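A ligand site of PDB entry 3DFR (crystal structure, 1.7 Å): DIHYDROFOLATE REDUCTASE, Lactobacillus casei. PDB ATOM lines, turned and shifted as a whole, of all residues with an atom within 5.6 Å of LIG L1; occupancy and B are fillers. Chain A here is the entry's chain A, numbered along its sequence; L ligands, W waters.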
ATOM      1  N   LEU A   4      30.582  17.261  -7.177  1.00  0.00           N
ATOM      2  CA  LEU A   4      29.426  16.526  -6.680  1.00  0.00           C
ATOM      3  C   LEU A   4      28.842  15.712  -7.841  1.00  0.00           C
ATOM      4  O   LEU A   4      28.496  16.270  -8.896  1.00  0.00           O
ATOM      5  CB  LEU A   4      28.383  17.644  -6.288  1.00  0.00           C
ATOM      6  CG  LEU A   4      26.914  17.138  -5.870  1.00  0.00           C
ATOM      7  CD1 LEU A   4      26.930  16.249  -4.651  1.00  0.00           C
ATOM      8  CD2 LEU A   4      26.081  18.453  -5.505  1.00  0.00           C
ATOM      9  N   TRP A   5      28.801  14.451  -7.669  1.00  0.00           N
ATOM     10  CA  TRP A   5      28.251  13.566  -8.744  1.00  0.00           C
ATOM     11  C   TRP A   5      27.685  12.244  -8.104  1.00  0.00           C
ATOM     12  O   TRP A   5      28.046  11.787  -7.080  1.00  0.00           O
ATOM     13  CB  TRP A   5      29.317  13.343  -9.908  1.00  0.00           C
ATOM     14  CG  TRP A   5      30.340  12.314  -9.615  1.00  0.00           C
ATOM     15  CD1 TRP A   5      30.301  11.023 -10.050  1.00  0.00           C
ATOM     16  CD2 TRP A   5      31.495  12.370  -8.769  1.00  0.00           C
ATOM     17  NE1 TRP A   5      31.457  10.277  -9.704  1.00  0.00           N
ATOM     18  CE2 TRP A   5      32.174  11.100  -8.934  1.00  0.00           C
ATOM     19  CE3 TRP A   5      32.052  13.418  -8.063  1.00  0.00           C
ATOM     20  CZ2 TRP A   5      33.386  10.849  -8.272  1.00  0.00           C
ATOM     21  CZ3 TRP A   5      33.207  13.068  -7.440  1.00  0.00           C
ATOM     22  CH2 TRP A   5      33.983  11.830  -7.450  1.00  0.00           C
ATOM     23  N   ALA A   6      26.905  11.625  -9.069  1.00  0.00           N
ATOM     24  CA  ALA A   6      26.373  10.206  -8.731  1.00  0.00           C
ATOM     25  C   ALA A   6      26.867   9.330  -9.873  1.00  0.00           C
ATOM     26  O   ALA A   6      26.752   9.778 -11.039  1.00  0.00           O
ATOM     27  CB  ALA A   6      24.827  10.276  -8.718  1.00  0.00           C
ATOM     28  N   LEU A  19      20.251  11.413 -17.150  1.00  0.00           N
ATOM     29  CA  LEU A  19      20.693  10.528 -16.160  1.00  0.00           C
ATOM     30  C   LEU A  19      20.176   9.174 -16.729  1.00  0.00           C
ATOM     31  O   LEU A  19      19.397   8.777 -17.389  1.00  0.00           O
ATOM     32  CB  LEU A  19      20.316  10.681 -14.728  1.00  0.00           C
ATOM     33  CG  LEU A  19      20.735  12.118 -14.291  1.00  0.00           C
ATOM     34  CD1 LEU A  19      19.955  12.218 -13.003  1.00  0.00           C
ATOM     35  CD2 LEU A  19      22.118  12.210 -13.951  1.00  0.00           C
ATOM     36  N   PRO A  24      15.206   9.458  -6.804  1.00  0.00           N
ATOM     37  CA  PRO A  24      14.797  10.679  -6.030  1.00  0.00           C
ATOM     38  C   PRO A  24      15.618  10.852  -4.785  1.00  0.00           C
ATOM     39  O   PRO A  24      15.772  12.098  -4.561  1.00  0.00           O
ATOM     40  CB  PRO A  24      13.255  10.436  -5.508  1.00  0.00           C
ATOM     41  CG  PRO A  24      12.753   9.997  -6.839  1.00  0.00           C
ATOM     42  CD  PRO A  24      13.608   8.706  -6.968  1.00  0.00           C
ATOM     43  N   ASP A  26      18.584  10.774  -4.087  1.00  0.00           N
ATOM     44  CA  ASP A  26      19.882  11.447  -4.510  1.00  0.00           C
ATOM     45  C   ASP A  26      19.666  12.832  -4.942  1.00  0.00           C
ATOM     46  O   ASP A  26      20.410  13.892  -4.922  1.00  0.00           O
ATOM     47  CB  ASP A  26      20.614  10.509  -5.541  1.00  0.00           C
ATOM     48  CG  ASP A  26      21.791  11.257  -6.228  1.00  0.00           C
ATOM     49  OD1 ASP A  26      21.777  11.781  -7.344  1.00  0.00           O
ATOM     50  OD2 ASP A  26      22.867  11.470  -5.465  1.00  0.00           O
ATOM     51  N   LEU A  27      18.534  13.124  -5.665  1.00  0.00           N
ATOM     52  CA  LEU A  27      18.145  14.481  -6.078  1.00  0.00           C
ATOM     53  C   LEU A  27      17.833  15.261  -4.763  1.00  0.00           C
ATOM     54  O   LEU A  27      18.236  16.427  -4.942  1.00  0.00           O
ATOM     55  CB  LEU A  27      16.915  14.475  -7.046  1.00  0.00           C
ATOM     56  CG  LEU A  27      17.059  13.866  -8.374  1.00  0.00           C
ATOM     57  CD1 LEU A  27      15.724  13.815  -9.254  1.00  0.00           C
ATOM     58  CD2 LEU A  27      18.158  14.278  -9.288  1.00  0.00           C
ATOM     59  N   HIS A  28      17.260  14.713  -3.692  1.00  0.00           N
ATOM     60  CA  HIS A  28      16.992  15.663  -2.575  1.00  0.00           C
ATOM     61  C   HIS A  28      18.422  15.736  -2.028  1.00  0.00           C
ATOM     62  O   HIS A  28      18.658  16.851  -1.502  1.00  0.00           O
ATOM     63  CB  HIS A  28      16.160  14.865  -1.498  1.00  0.00           C
ATOM     64  CG  HIS A  28      14.822  14.397  -2.115  1.00  0.00           C
ATOM     65  ND1 HIS A  28      14.029  14.766  -3.131  1.00  0.00           N
ATOM     66  CD2 HIS A  28      14.218  13.101  -1.603  1.00  0.00           C
ATOM     67  CE1 HIS A  28      13.011  13.906  -3.321  1.00  0.00           C
ATOM     68  NE2 HIS A  28      13.100  12.892  -2.422  1.00  0.00           N
ATOM     69  N   TYR A  29      19.411  14.890  -2.018  1.00  0.00           N
ATOM     70  CA  TYR A  29      20.739  15.136  -1.442  1.00  0.00           C
ATOM     71  C   TYR A  29      21.437  16.257  -2.275  1.00  0.00           C
ATOM     72  O   TYR A  29      22.154  17.055  -1.749  1.00  0.00           O
ATOM     73  CB  TYR A  29      21.477  13.819  -1.583  1.00  0.00           C
ATOM     74  CG  TYR A  29      22.899  13.954  -1.169  1.00  0.00           C
ATOM     75  CD1 TYR A  29      23.260  13.894   0.205  1.00  0.00           C
ATOM     76  CD2 TYR A  29      24.033  13.953  -1.927  1.00  0.00           C
ATOM     77  CE1 TYR A  29      24.572  13.848   0.754  1.00  0.00           C
ATOM     78  CE2 TYR A  29      25.376  13.917  -1.567  1.00  0.00           C
ATOM     79  CZ  TYR A  29      25.605  13.962  -0.130  1.00  0.00           C
ATOM     80  OH  TYR A  29      26.884  13.878   0.448  1.00  0.00           O
ATOM     81  N   PHE A  30      21.331  16.150  -3.656  1.00  0.00           N
ATOM     82  CA  PHE A  30      21.873  17.221  -4.551  1.00  0.00           C
ATOM     83  C   PHE A  30      21.486  18.665  -4.092  1.00  0.00           C
ATOM     84  O   PHE A  30      22.219  19.538  -4.189  1.00  0.00           O
ATOM     85  CB  PHE A  30      21.412  16.841  -6.075  1.00  0.00           C
ATOM     86  CG  PHE A  30      21.890  17.799  -7.044  1.00  0.00           C
ATOM     87  CD1 PHE A  30      20.985  18.847  -7.330  1.00  0.00           C
ATOM     88  CD2 PHE A  30      23.127  17.820  -7.556  1.00  0.00           C
ATOM     89  CE1 PHE A  30      21.320  19.925  -8.217  1.00  0.00           C
ATOM     90  CE2 PHE A  30      23.514  18.818  -8.551  1.00  0.00           C
ATOM     91  CZ  PHE A  30      22.539  19.798  -8.812  1.00  0.00           C
ATOM     92  N   ARG A  31      20.143  18.663  -3.946  1.00  0.00           N
ATOM     93  CA  ARG A  31      19.611  20.007  -3.492  1.00  0.00           C
ATOM     94  C   ARG A  31      20.273  20.382  -2.144  1.00  0.00           C
ATOM     95  O   ARG A  31      20.723  21.543  -1.951  1.00  0.00           O
ATOM     96  CB  ARG A  31      18.092  19.843  -3.361  1.00  0.00           C
ATOM     97  CG  ARG A  31      17.478  21.228  -2.845  1.00  0.00           C
ATOM     98  CD  ARG A  31      15.869  21.333  -2.707  1.00  0.00           C
ATOM     99  NE  ARG A  31      15.142  22.194  -1.686  1.00  0.00           N
ATOM    100  CZ  ARG A  31      14.995  23.584  -2.156  1.00  0.00           C
ATOM    101  NH1 ARG A  31      14.844  24.012  -3.452  1.00  0.00           N
ATOM    102  NH2 ARG A  31      15.069  24.414  -1.006  1.00  0.00           N
ATOM    103  N   THR A  34      23.567  21.856  -2.589  1.00  0.00           N
ATOM    104  CA  THR A  34      23.985  22.907  -3.506  1.00  0.00           C
ATOM    105  C   THR A  34      23.174  24.209  -3.105  1.00  0.00           C
ATOM    106  O   THR A  34      23.682  25.206  -3.598  1.00  0.00           O
ATOM    107  CB  THR A  34      23.606  22.626  -5.031  1.00  0.00           C
ATOM    108  OG1 THR A  34      22.318  22.076  -5.119  1.00  0.00           O
ATOM    109  CG2 THR A  34      24.561  21.528  -5.628  1.00  0.00           C
ATOM    110  N   THR A  45      24.316  19.935 -19.301  1.00  0.00           N
ATOM    111  CA  THR A  45      23.716  19.496 -17.966  1.00  0.00           C
ATOM    112  C   THR A  45      22.775  20.781 -17.684  1.00  0.00           C
ATOM    113  O   THR A  45      21.663  20.394 -17.276  1.00  0.00           O
ATOM    114  CB  THR A  45      24.741  19.432 -16.761  1.00  0.00           C
ATOM    115  OG1 THR A  45      25.535  18.360 -17.350  1.00  0.00           O
ATOM    116  CG2 THR A  45      24.149  19.218 -15.370  1.00  0.00           C
ATOM    117  N   SER A  48      19.163  20.213 -19.385  1.00  0.00           N
ATOM    118  CA  SER A  48      18.559  18.948 -18.830  1.00  0.00           C
ATOM    119  C   SER A  48      17.858  19.060 -17.500  1.00  0.00           C
ATOM    120  O   SER A  48      17.162  18.270 -16.982  1.00  0.00           O
ATOM    121  CB  SER A  48      19.590  17.865 -18.603  1.00  0.00           C
ATOM    122  OG  SER A  48      20.367  17.941 -17.405  1.00  0.00           O
ATOM    123  N   PHE A  49      18.153  20.237 -16.727  1.00  0.00           N
ATOM    124  CA  PHE A  49      17.365  20.567 -15.481  1.00  0.00           C
ATOM    125  C   PHE A  49      15.811  20.802 -15.947  1.00  0.00           C
ATOM    126  O   PHE A  49      15.585  21.549 -16.853  1.00  0.00           O
ATOM    127  CB  PHE A  49      17.908  21.679 -14.668  1.00  0.00           C
ATOM    128  CG  PHE A  49      19.365  21.498 -14.232  1.00  0.00           C
ATOM    129  CD1 PHE A  49      20.148  20.469 -13.860  1.00  0.00           C
ATOM    130  CD2 PHE A  49      19.938  22.896 -13.909  1.00  0.00           C
ATOM    131  CE1 PHE A  49      21.313  20.500 -13.256  1.00  0.00           C
ATOM    132  CE2 PHE A  49      21.276  22.894 -13.265  1.00  0.00           C
ATOM    133  CZ  PHE A  49      21.933  21.668 -13.012  1.00  0.00           C
ATOM    134  N   PRO A  50      15.077  20.086 -14.865  1.00  0.00           N
ATOM    135  CA  PRO A  50      13.579  20.388 -15.335  1.00  0.00           C
ATOM    136  C   PRO A  50      13.077  21.798 -15.121  1.00  0.00           C
ATOM    137  O   PRO A  50      12.146  22.139 -15.807  1.00  0.00           O
ATOM    138  CB  PRO A  50      12.581  19.703 -14.162  1.00  0.00           C
ATOM    139  CG  PRO A  50      13.571  18.753 -13.614  1.00  0.00           C
ATOM    140  CD  PRO A  50      14.816  19.472 -13.206  1.00  0.00           C
ATOM    141  N   LEU A  54      17.916  26.498 -11.242  1.00  0.00           N
ATOM    142  CA  LEU A  54      17.491  25.699 -10.066  1.00  0.00           C
ATOM    143  C   LEU A  54      17.556  26.889  -9.048  1.00  0.00           C
ATOM    144  O   LEU A  54      18.328  27.650  -8.733  1.00  0.00           O
ATOM    145  CB  LEU A  54      18.407  24.481  -9.664  1.00  0.00           C
ATOM    146  CG  LEU A  54      18.192  23.269 -10.677  1.00  0.00           C
ATOM    147  CD1 LEU A  54      19.294  22.273 -10.041  1.00  0.00           C
ATOM    148  CD2 LEU A  54      16.883  22.728 -10.477  1.00  0.00           C
ATOM    149  N   PRO A  55      16.244  26.636  -8.216  1.00  0.00           N
ATOM    150  CA  PRO A  55      16.240  27.876  -7.283  1.00  0.00           C
ATOM    151  C   PRO A  55      16.994  27.836  -6.029  1.00  0.00           C
ATOM    152  O   PRO A  55      17.484  26.717  -5.613  1.00  0.00           O
ATOM    153  CB  PRO A  55      14.758  27.902  -6.726  1.00  0.00           C
ATOM    154  CG  PRO A  55      14.446  26.411  -6.576  1.00  0.00           C
ATOM    155  CD  PRO A  55      14.653  26.115  -8.033  1.00  0.00           C
ATOM    156  N   ARG A  57      20.174  28.883  -5.262  1.00  0.00           N
ATOM    157  CA  ARG A  57      21.616  28.616  -5.268  1.00  0.00           C
ATOM    158  C   ARG A  57      21.941  29.472  -6.533  1.00  0.00           C
ATOM    159  O   ARG A  57      21.125  29.757  -7.451  1.00  0.00           O
ATOM    160  CB  ARG A  57      21.936  27.017  -5.563  1.00  0.00           C
ATOM    161  CG  ARG A  57      21.414  26.517  -6.984  1.00  0.00           C
ATOM    162  CD  ARG A  57      21.218  25.048  -6.609  1.00  0.00           C
ATOM    163  NE  ARG A  57      19.941  24.975  -5.971  1.00  0.00           N
ATOM    164  CZ  ARG A  57      19.116  23.992  -5.966  1.00  0.00           C
ATOM    165  NH1 ARG A  57      19.623  22.711  -6.233  1.00  0.00           N
ATOM    166  NH2 ARG A  57      17.782  24.020  -5.980  1.00  0.00           N
ATOM    167  N   ILE A  96      31.136  22.041  -8.170  1.00  0.00           N
ATOM    168  CA  ILE A  96      31.165  21.675  -9.635  1.00  0.00           C
ATOM    169  C   ILE A  96      30.240  20.412  -9.696  1.00  0.00           C
ATOM    170  O   ILE A  96      30.505  19.494  -9.015  1.00  0.00           O
ATOM    171  CB  ILE A  96      32.658  21.506  -9.988  1.00  0.00           C
ATOM    172  CG1 ILE A  96      33.747  22.560  -9.516  1.00  0.00           C
ATOM    173  CG2 ILE A  96      32.537  21.277 -11.567  1.00  0.00           C
ATOM    174  CD1 ILE A  96      33.257  23.850 -10.105  1.00  0.00           C
ATOM    175  N   ALA A  97      29.140  20.637 -10.451  1.00  0.00           N
ATOM    176  CA  ALA A  97      28.118  19.587 -10.530  1.00  0.00           C
ATOM    177  C   ALA A  97      28.101  18.831 -11.956  1.00  0.00           C
ATOM    178  O   ALA A  97      27.141  18.057 -11.994  1.00  0.00           O
ATOM    179  CB  ALA A  97      26.805  20.311 -10.126  1.00  0.00           C
ATOM    180  N   GLY A  98      29.069  19.059 -12.801  1.00  0.00           N
ATOM    181  CA  GLY A  98      29.099  18.373 -14.027  1.00  0.00           C
ATOM    182  C   GLY A  98      28.703  19.061 -15.257  1.00  0.00           C
ATOM    183  O   GLY A  98      28.326  20.138 -15.103  1.00  0.00           O
ATOM    184  N   PHE A 103      33.764  18.641 -15.381  1.00  0.00           N
ATOM    185  CA  PHE A 103      34.698  18.040 -14.383  1.00  0.00           C
ATOM    186  C   PHE A 103      36.159  18.086 -14.842  1.00  0.00           C
ATOM    187  O   PHE A 103      37.121  18.308 -14.129  1.00  0.00           O
ATOM    188  CB  PHE A 103      34.261  16.608 -14.004  1.00  0.00           C
ATOM    189  CG  PHE A 103      32.922  16.451 -13.205  1.00  0.00           C
ATOM    190  CD1 PHE A 103      32.861  17.329 -12.051  1.00  0.00           C
ATOM    191  CD2 PHE A 103      31.935  15.569 -13.629  1.00  0.00           C
ATOM    192  CE1 PHE A 103      31.720  17.068 -11.273  1.00  0.00           C
ATOM    193  CE2 PHE A 103      30.803  15.372 -12.822  1.00  0.00           C
ATOM    194  CZ  PHE A 103      30.693  16.283 -11.709  1.00  0.00           C
ATOM    195  N   LEU A 114      32.165  14.750  -3.434  1.00  0.00           N
ATOM    196  CA  LEU A 114      30.828  14.377  -2.876  1.00  0.00           C
ATOM    197  C   LEU A 114      30.303  13.356  -3.965  1.00  0.00           C
ATOM    198  O   LEU A 114      29.762  13.820  -4.950  1.00  0.00           O
ATOM    199  CB  LEU A 114      29.900  15.576  -2.667  1.00  0.00           C
ATOM    200  CG  LEU A 114      30.782  16.578  -1.778  1.00  0.00           C
ATOM    201  CD1 LEU A 114      29.941  17.810  -1.898  1.00  0.00           C
ATOM    202  CD2 LEU A 114      30.843  16.153  -0.360  1.00  0.00           C
ATOM    203  N   THR A 116      27.966   9.881  -4.979  1.00  0.00           N
ATOM    204  CA  THR A 116      26.947   8.922  -4.605  1.00  0.00           C
ATOM    205  C   THR A 116      27.328   7.702  -5.542  1.00  0.00           C
ATOM    206  O   THR A 116      27.366   7.868  -6.741  1.00  0.00           O
ATOM    207  CB  THR A 116      25.584   9.335  -5.066  1.00  0.00           C
ATOM    208  OG1 THR A 116      25.272  10.674  -4.494  1.00  0.00           O
ATOM    209  CG2 THR A 116      24.367   8.405  -4.571  1.00  0.00           C
HETATM  210  N1  LIG L   1      23.262  13.753  -8.249  1.00  0.00           N
HETATM  211  C1  LIG L   1      24.467  14.090  -7.628  1.00  0.00           C
HETATM  212  N2  LIG L   1      24.725  13.448  -6.444  1.00  0.00           N
HETATM  213  N3  LIG L   1      25.330  14.958  -8.185  1.00  0.00           N
HETATM  214  C2  LIG L   1      25.144  15.682  -9.323  1.00  0.00           C
HETATM  215  N4  LIG L   1      25.979  16.561  -9.821  1.00  0.00           N
HETATM  216  C3  LIG L   1      23.839  15.402  -9.961  1.00  0.00           C
HETATM  217  N5  LIG L   1      23.455  16.104 -11.047  1.00  0.00           N
HETATM  218  C4  LIG L   1      22.269  15.784 -11.568  1.00  0.00           C
HETATM  219  C5  LIG L   1      21.552  14.748 -10.977  1.00  0.00           C
HETATM  220  N6  LIG L   1      21.765  14.106  -9.973  1.00  0.00           N
HETATM  221  C6  LIG L   1      22.983  14.403  -9.421  1.00  0.00           C
HETATM  222  C7  LIG L   1      21.974  16.483 -12.908  1.00  0.00           C
HETATM  223  N7  LIG L   1      20.625  16.567 -13.156  1.00  0.00           N
HETATM  224  C8  LIG L   1      20.256  15.966 -14.501  1.00  0.00           C
HETATM  225  C9  LIG L   1      17.697  18.242 -10.708  1.00  0.00           C
HETATM  226  C10 LIG L   1      17.334  17.459 -11.789  1.00  0.00           C
HETATM  227  C11 LIG L   1      18.076  16.860 -12.754  1.00  0.00           C
HETATM  228  C12 LIG L   1      19.579  17.099 -12.460  1.00  0.00           C
HETATM  229  C13 LIG L   1      19.910  17.842 -11.219  1.00  0.00           C
HETATM  230  C14 LIG L   1      19.070  18.293 -10.359  1.00  0.00           C
HETATM  231  C15 LIG L   1      16.698  18.597  -9.949  1.00  0.00           C
HETATM  232  O1  LIG L   1      15.475  18.657 -10.033  1.00  0.00           O
HETATM  233  N8  LIG L   1      16.717  18.817  -8.656  1.00  0.00           N
HETATM  234  C16 LIG L   1      16.085  19.482  -7.645  1.00  0.00           C
HETATM  235  C17 LIG L   1      17.018  20.475  -6.976  1.00  0.00           C
HETATM  236  O2  LIG L   1      18.209  20.484  -6.715  1.00  0.00           O
HETATM  237  O3  LIG L   1      16.239  21.436  -6.365  1.00  0.00           O
HETATM  238  C18 LIG L   1      15.466  18.821  -6.353  1.00  0.00           C
HETATM  239  C19 LIG L   1      14.270  17.955  -6.464  1.00  0.00           C
HETATM  240  C20 LIG L   1      13.806  16.492  -5.810  1.00  0.00           C
HETATM  241  O4  LIG L   1      12.891  15.650  -6.382  1.00  0.00           O
HETATM  242  O5  LIG L   1      14.334  16.954  -4.686  1.00  0.00           O
HETATM  243  P1  LG2 L   2      28.593  19.132 -19.825  1.00  0.00           P
HETATM  244  O1  LG2 L   2      29.921  19.039 -19.168  1.00  0.00           O
HETATM  245  O2  LG2 L   2      27.405  19.208 -18.952  1.00  0.00           O
HETATM  246  O3  LG2 L   2      28.431  20.331 -20.945  1.00  0.00           O
HETATM  247  C1  LG2 L   2      29.469  20.580 -22.022  1.00  0.00           C
HETATM  248  C2  LG2 L   2      29.187  22.039 -22.595  1.00  0.00           C
HETATM  249  O4  LG2 L   2      29.873  22.737 -21.718  1.00  0.00           O
HETATM  250  C3  LG2 L   2      30.102  22.127 -23.901  1.00  0.00           C
HETATM  251  O5  LG2 L   2      29.187  21.524 -24.904  1.00  0.00           O
HETATM  252  C4  LG2 L   2      30.184  23.716 -23.753  1.00  0.00           C
HETATM  253  O6  LG2 L   2      28.896  24.226 -24.099  1.00  0.00           O
HETATM  254  C5  LG2 L   2      30.509  23.934 -22.305  1.00  0.00           C
HETATM  255  N1  LG2 L   2      31.895  23.857 -22.018  1.00  0.00           N
HETATM  256  C6  LG2 L   2      32.725  22.810 -21.777  1.00  0.00           C
HETATM  257  N2  LG2 L   2      33.893  22.994 -21.319  1.00  0.00           N
HETATM  258  C7  LG2 L   2      34.010  24.409 -21.521  1.00  0.00           C
HETATM  259  C8  LG2 L   2      35.166  25.397 -21.107  1.00  0.00           C
HETATM  260  N3  LG2 L   2      36.336  24.968 -20.624  1.00  0.00           N
HETATM  261  N4  LG2 L   2      34.748  26.580 -21.224  1.00  0.00           N
HETATM  262  C9  LG2 L   2      33.435  26.916 -21.574  1.00  0.00           C
HETATM  263  N5  LG2 L   2      32.375  26.199 -22.037  1.00  0.00           N
HETATM  264  C10 LG2 L   2      32.749  24.866 -21.771  1.00  0.00           C
HETATM  265  O7  LG2 L   2      28.292  17.894 -20.782  1.00  0.00           O
HETATM  266  P2  LG2 L   2      28.896  16.409 -20.953  1.00  0.00           P
HETATM  267  O8  LG2 L   2      30.282  16.270 -20.607  1.00  0.00           O
HETATM  268  O9  LG2 L   2      28.113  15.818 -22.129  1.00  0.00           O
HETATM  269  O10 LG2 L   2      27.993  15.762 -19.743  1.00  0.00           O
HETATM  270  C11 LG2 L   2      26.490  15.762 -19.628  1.00  0.00           C
HETATM  271  C12 LG2 L   2      26.159  14.274 -19.350  1.00  0.00           C
HETATM  272  O11 LG2 L   2      26.532  14.060 -17.923  1.00  0.00           O
HETATM  273  C13 LG2 L   2      24.632  14.088 -19.403  1.00  0.00           C
HETATM  274  O12 LG2 L   2      24.247  12.735 -19.682  1.00  0.00           O
HETATM  275  C14 LG2 L   2      24.261  14.384 -17.955  1.00  0.00           C
HETATM  276  O13 LG2 L   2      22.981  13.774 -17.632  1.00  0.00           O
HETATM  277  C15 LG2 L   2      25.394  13.770 -17.138  1.00  0.00           C
HETATM  278  N6  LG2 L   2      25.509  14.185 -15.663  1.00  0.00           N
HETATM  279  C16 LG2 L   2      25.390  13.459 -14.562  1.00  0.00           C
HETATM  280  C17 LG2 L   2      25.875  13.747 -13.400  1.00  0.00           C
HETATM  281  C18 LG2 L   2      25.561  12.682 -12.499  1.00  0.00           C
HETATM  282  O14 LG2 L   2      26.021  13.136 -11.351  1.00  0.00           O
HETATM  283  N7  LG2 L   2      25.337  11.370 -12.758  1.00  0.00           N
HETATM  284  C19 LG2 L   2      26.111  15.200 -13.161  1.00  0.00           C
HETATM  285  C20 LG2 L   2      26.061  16.077 -14.301  1.00  0.00           C
HETATM  286  C21 LG2 L   2      25.772  15.614 -15.576  1.00  0.00           C
HETATM  287  P3  LG2 L   2      28.433  24.944 -25.533  1.00  0.00           P
HETATM  288  O15 LG2 L   2      27.078  25.516 -25.126  1.00  0.00           O
HETATM  289  O16 LG2 L   2      29.747  25.600 -25.951  1.00  0.00           O
HETATM  290  O17 LG2 L   2      28.219  23.616 -26.364  1.00  0.00           O
HETATM  291  O   HOH W   1      11.015  16.088  -4.685  1.00  0.00           O
HETATM  292  O   HOH W   2      13.654  19.316  -3.822  1.00  0.00           O
HETATM  293  O   HOH W   3      13.161  19.794 -10.377  1.00  0.00           O
HETATM  294  O   HOH W   4      13.520  16.945 -10.254  1.00  0.00           O
HETATM  295  O   HOH W   5      22.625  16.486 -16.441  1.00  0.00           O
HETATM  296  O   HOH W   6      13.915  17.782  -1.617  1.00  0.00           O
HETATM  297  O   HOH W   7      14.089  22.824  -7.112  1.00  0.00           O
HETATM  298  O   HOH W   8      20.582  11.046  -9.491  1.00  0.00           O
HETATM  299  O   HOH W   9      27.060  12.976  -4.140  1.00  0.00           O
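A ring nitrogen (ND1) of His 28 is in hydrogen-bond range of an oxygen (O5) of LIG L1.
An oxygen (O2) of LIG L1 lies within salt-bridge range of the guanidinium group (NH1) of Arg 57, at 2.7 Å.
O2 of LG2 L2 lies within hydrogen-bond range of OG1 of Thr 45 (2.6 Å).
The backbone carbonyl oxygen (O) of Leu 4 is in hydrogen-bond range of a nitrogen (N4) of LIG L1 (2.7 Å).
A nitrogen (N4) of LIG L1 lies within hydrogen-bond range of the backbone carbonyl oxygen of Ala 97, 2.9 Å away.
An oxygen (O14) of LG2 L2 is in hydrogen-bond range of the backbone NH (N) of Ala 6 (2.9 Å).
The backbone carbonyl oxygen of Ala 6 sits at hydrogen-bond distance from a nitrogen (N7) of LG2 L2, at 2.7 Å.
An oxygen (O2) of LG2 L2 sits at hydrogen-bond distance from the backbone NH of Thr 45 (3.2 Å).
A nitrogen (N2) of LIG L1 is in hydrogen-bond range of the side-chain hydroxyl (OG1) of Thr 116 (3.4 Å).
The side-chain carboxylate (OD1) of Asp 26 sits at hydrogen-bond distance from a nitrogen (N1) of LIG L1 (2.6 Å).
Water W5 bridges OG of Ser 48 (2.9 Å) and O13 of LG2 L2 (3.0 Å).
Water W6 lies within hydrogen-bond range of O5 of LIG L1 (3.2 Å) and ND1 of His 28 (3.4 Å).
Water W9 lies within hydrogen-bond range of OG1 of Thr 116 (2.9 Å), O of Leu 114 (2.9 Å), N2 of LIG L1 (3.3 Å) and O of Trp 5 (3.3 Å).
Water W8 lies within hydrogen-bond range of the side-chain carboxylate of Asp 26 (2.6 Å) and a nitrogen (N6) of LIG L1 (3.3 Å).
Residues that only touch LIG L1: Phe 30, Trp 5, Pro 50, Arg 31, Ser 48, Leu 19, Phe 49, Leu 27, Ala 6 and Leu 54.
16 residues have an atom within 4 Å of LIG L1: Leu 4, Trp 5, Ala 6, Leu 19, Asp 26, Leu 27, His 28, Phe 30, Arg 31, Ser 48, Phe 49, Pro 50, Leu 54, Arg 57, Ala 97 and Thr 116.
Along chain A the residues within 4 Å of LIG L1 span positions 4 to 116.
The backbone carbonyl oxygen (O) of Thr 45 is in hydrogen-bond range of the side-chain hydroxyl (OG) of Ser 48, at 2.8 Å.
ND1 of His 28 sits close to O of Pro 24, 3.5 Å away.
NH1 of Arg 57 is in hydrogen-bond range of OG1 of Thr 34, 3.0 Å away.
The side-chain carboxylate (OD2) of Asp 26 is in hydrogen-bond range of the side-chain hydroxyl (OG1) of Thr 116, at 2.7 Å.
The guanidinium group (NH2) of Arg 57 lies within hydrogen-bond range of the backbone carbonyl oxygen (O) of Pro 55, 2.7 Å away.
The backbone carbonyl oxygen (O) of Leu 114 lies within hydrogen-bond range of the backbone NH (N) of Trp 5.
O of Trp 5 sits at hydrogen-bond distance from N of Thr 116.
OG1 of Thr 34 sits at hydrogen-bond distance from O of Phe 30 (2.7 Å).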
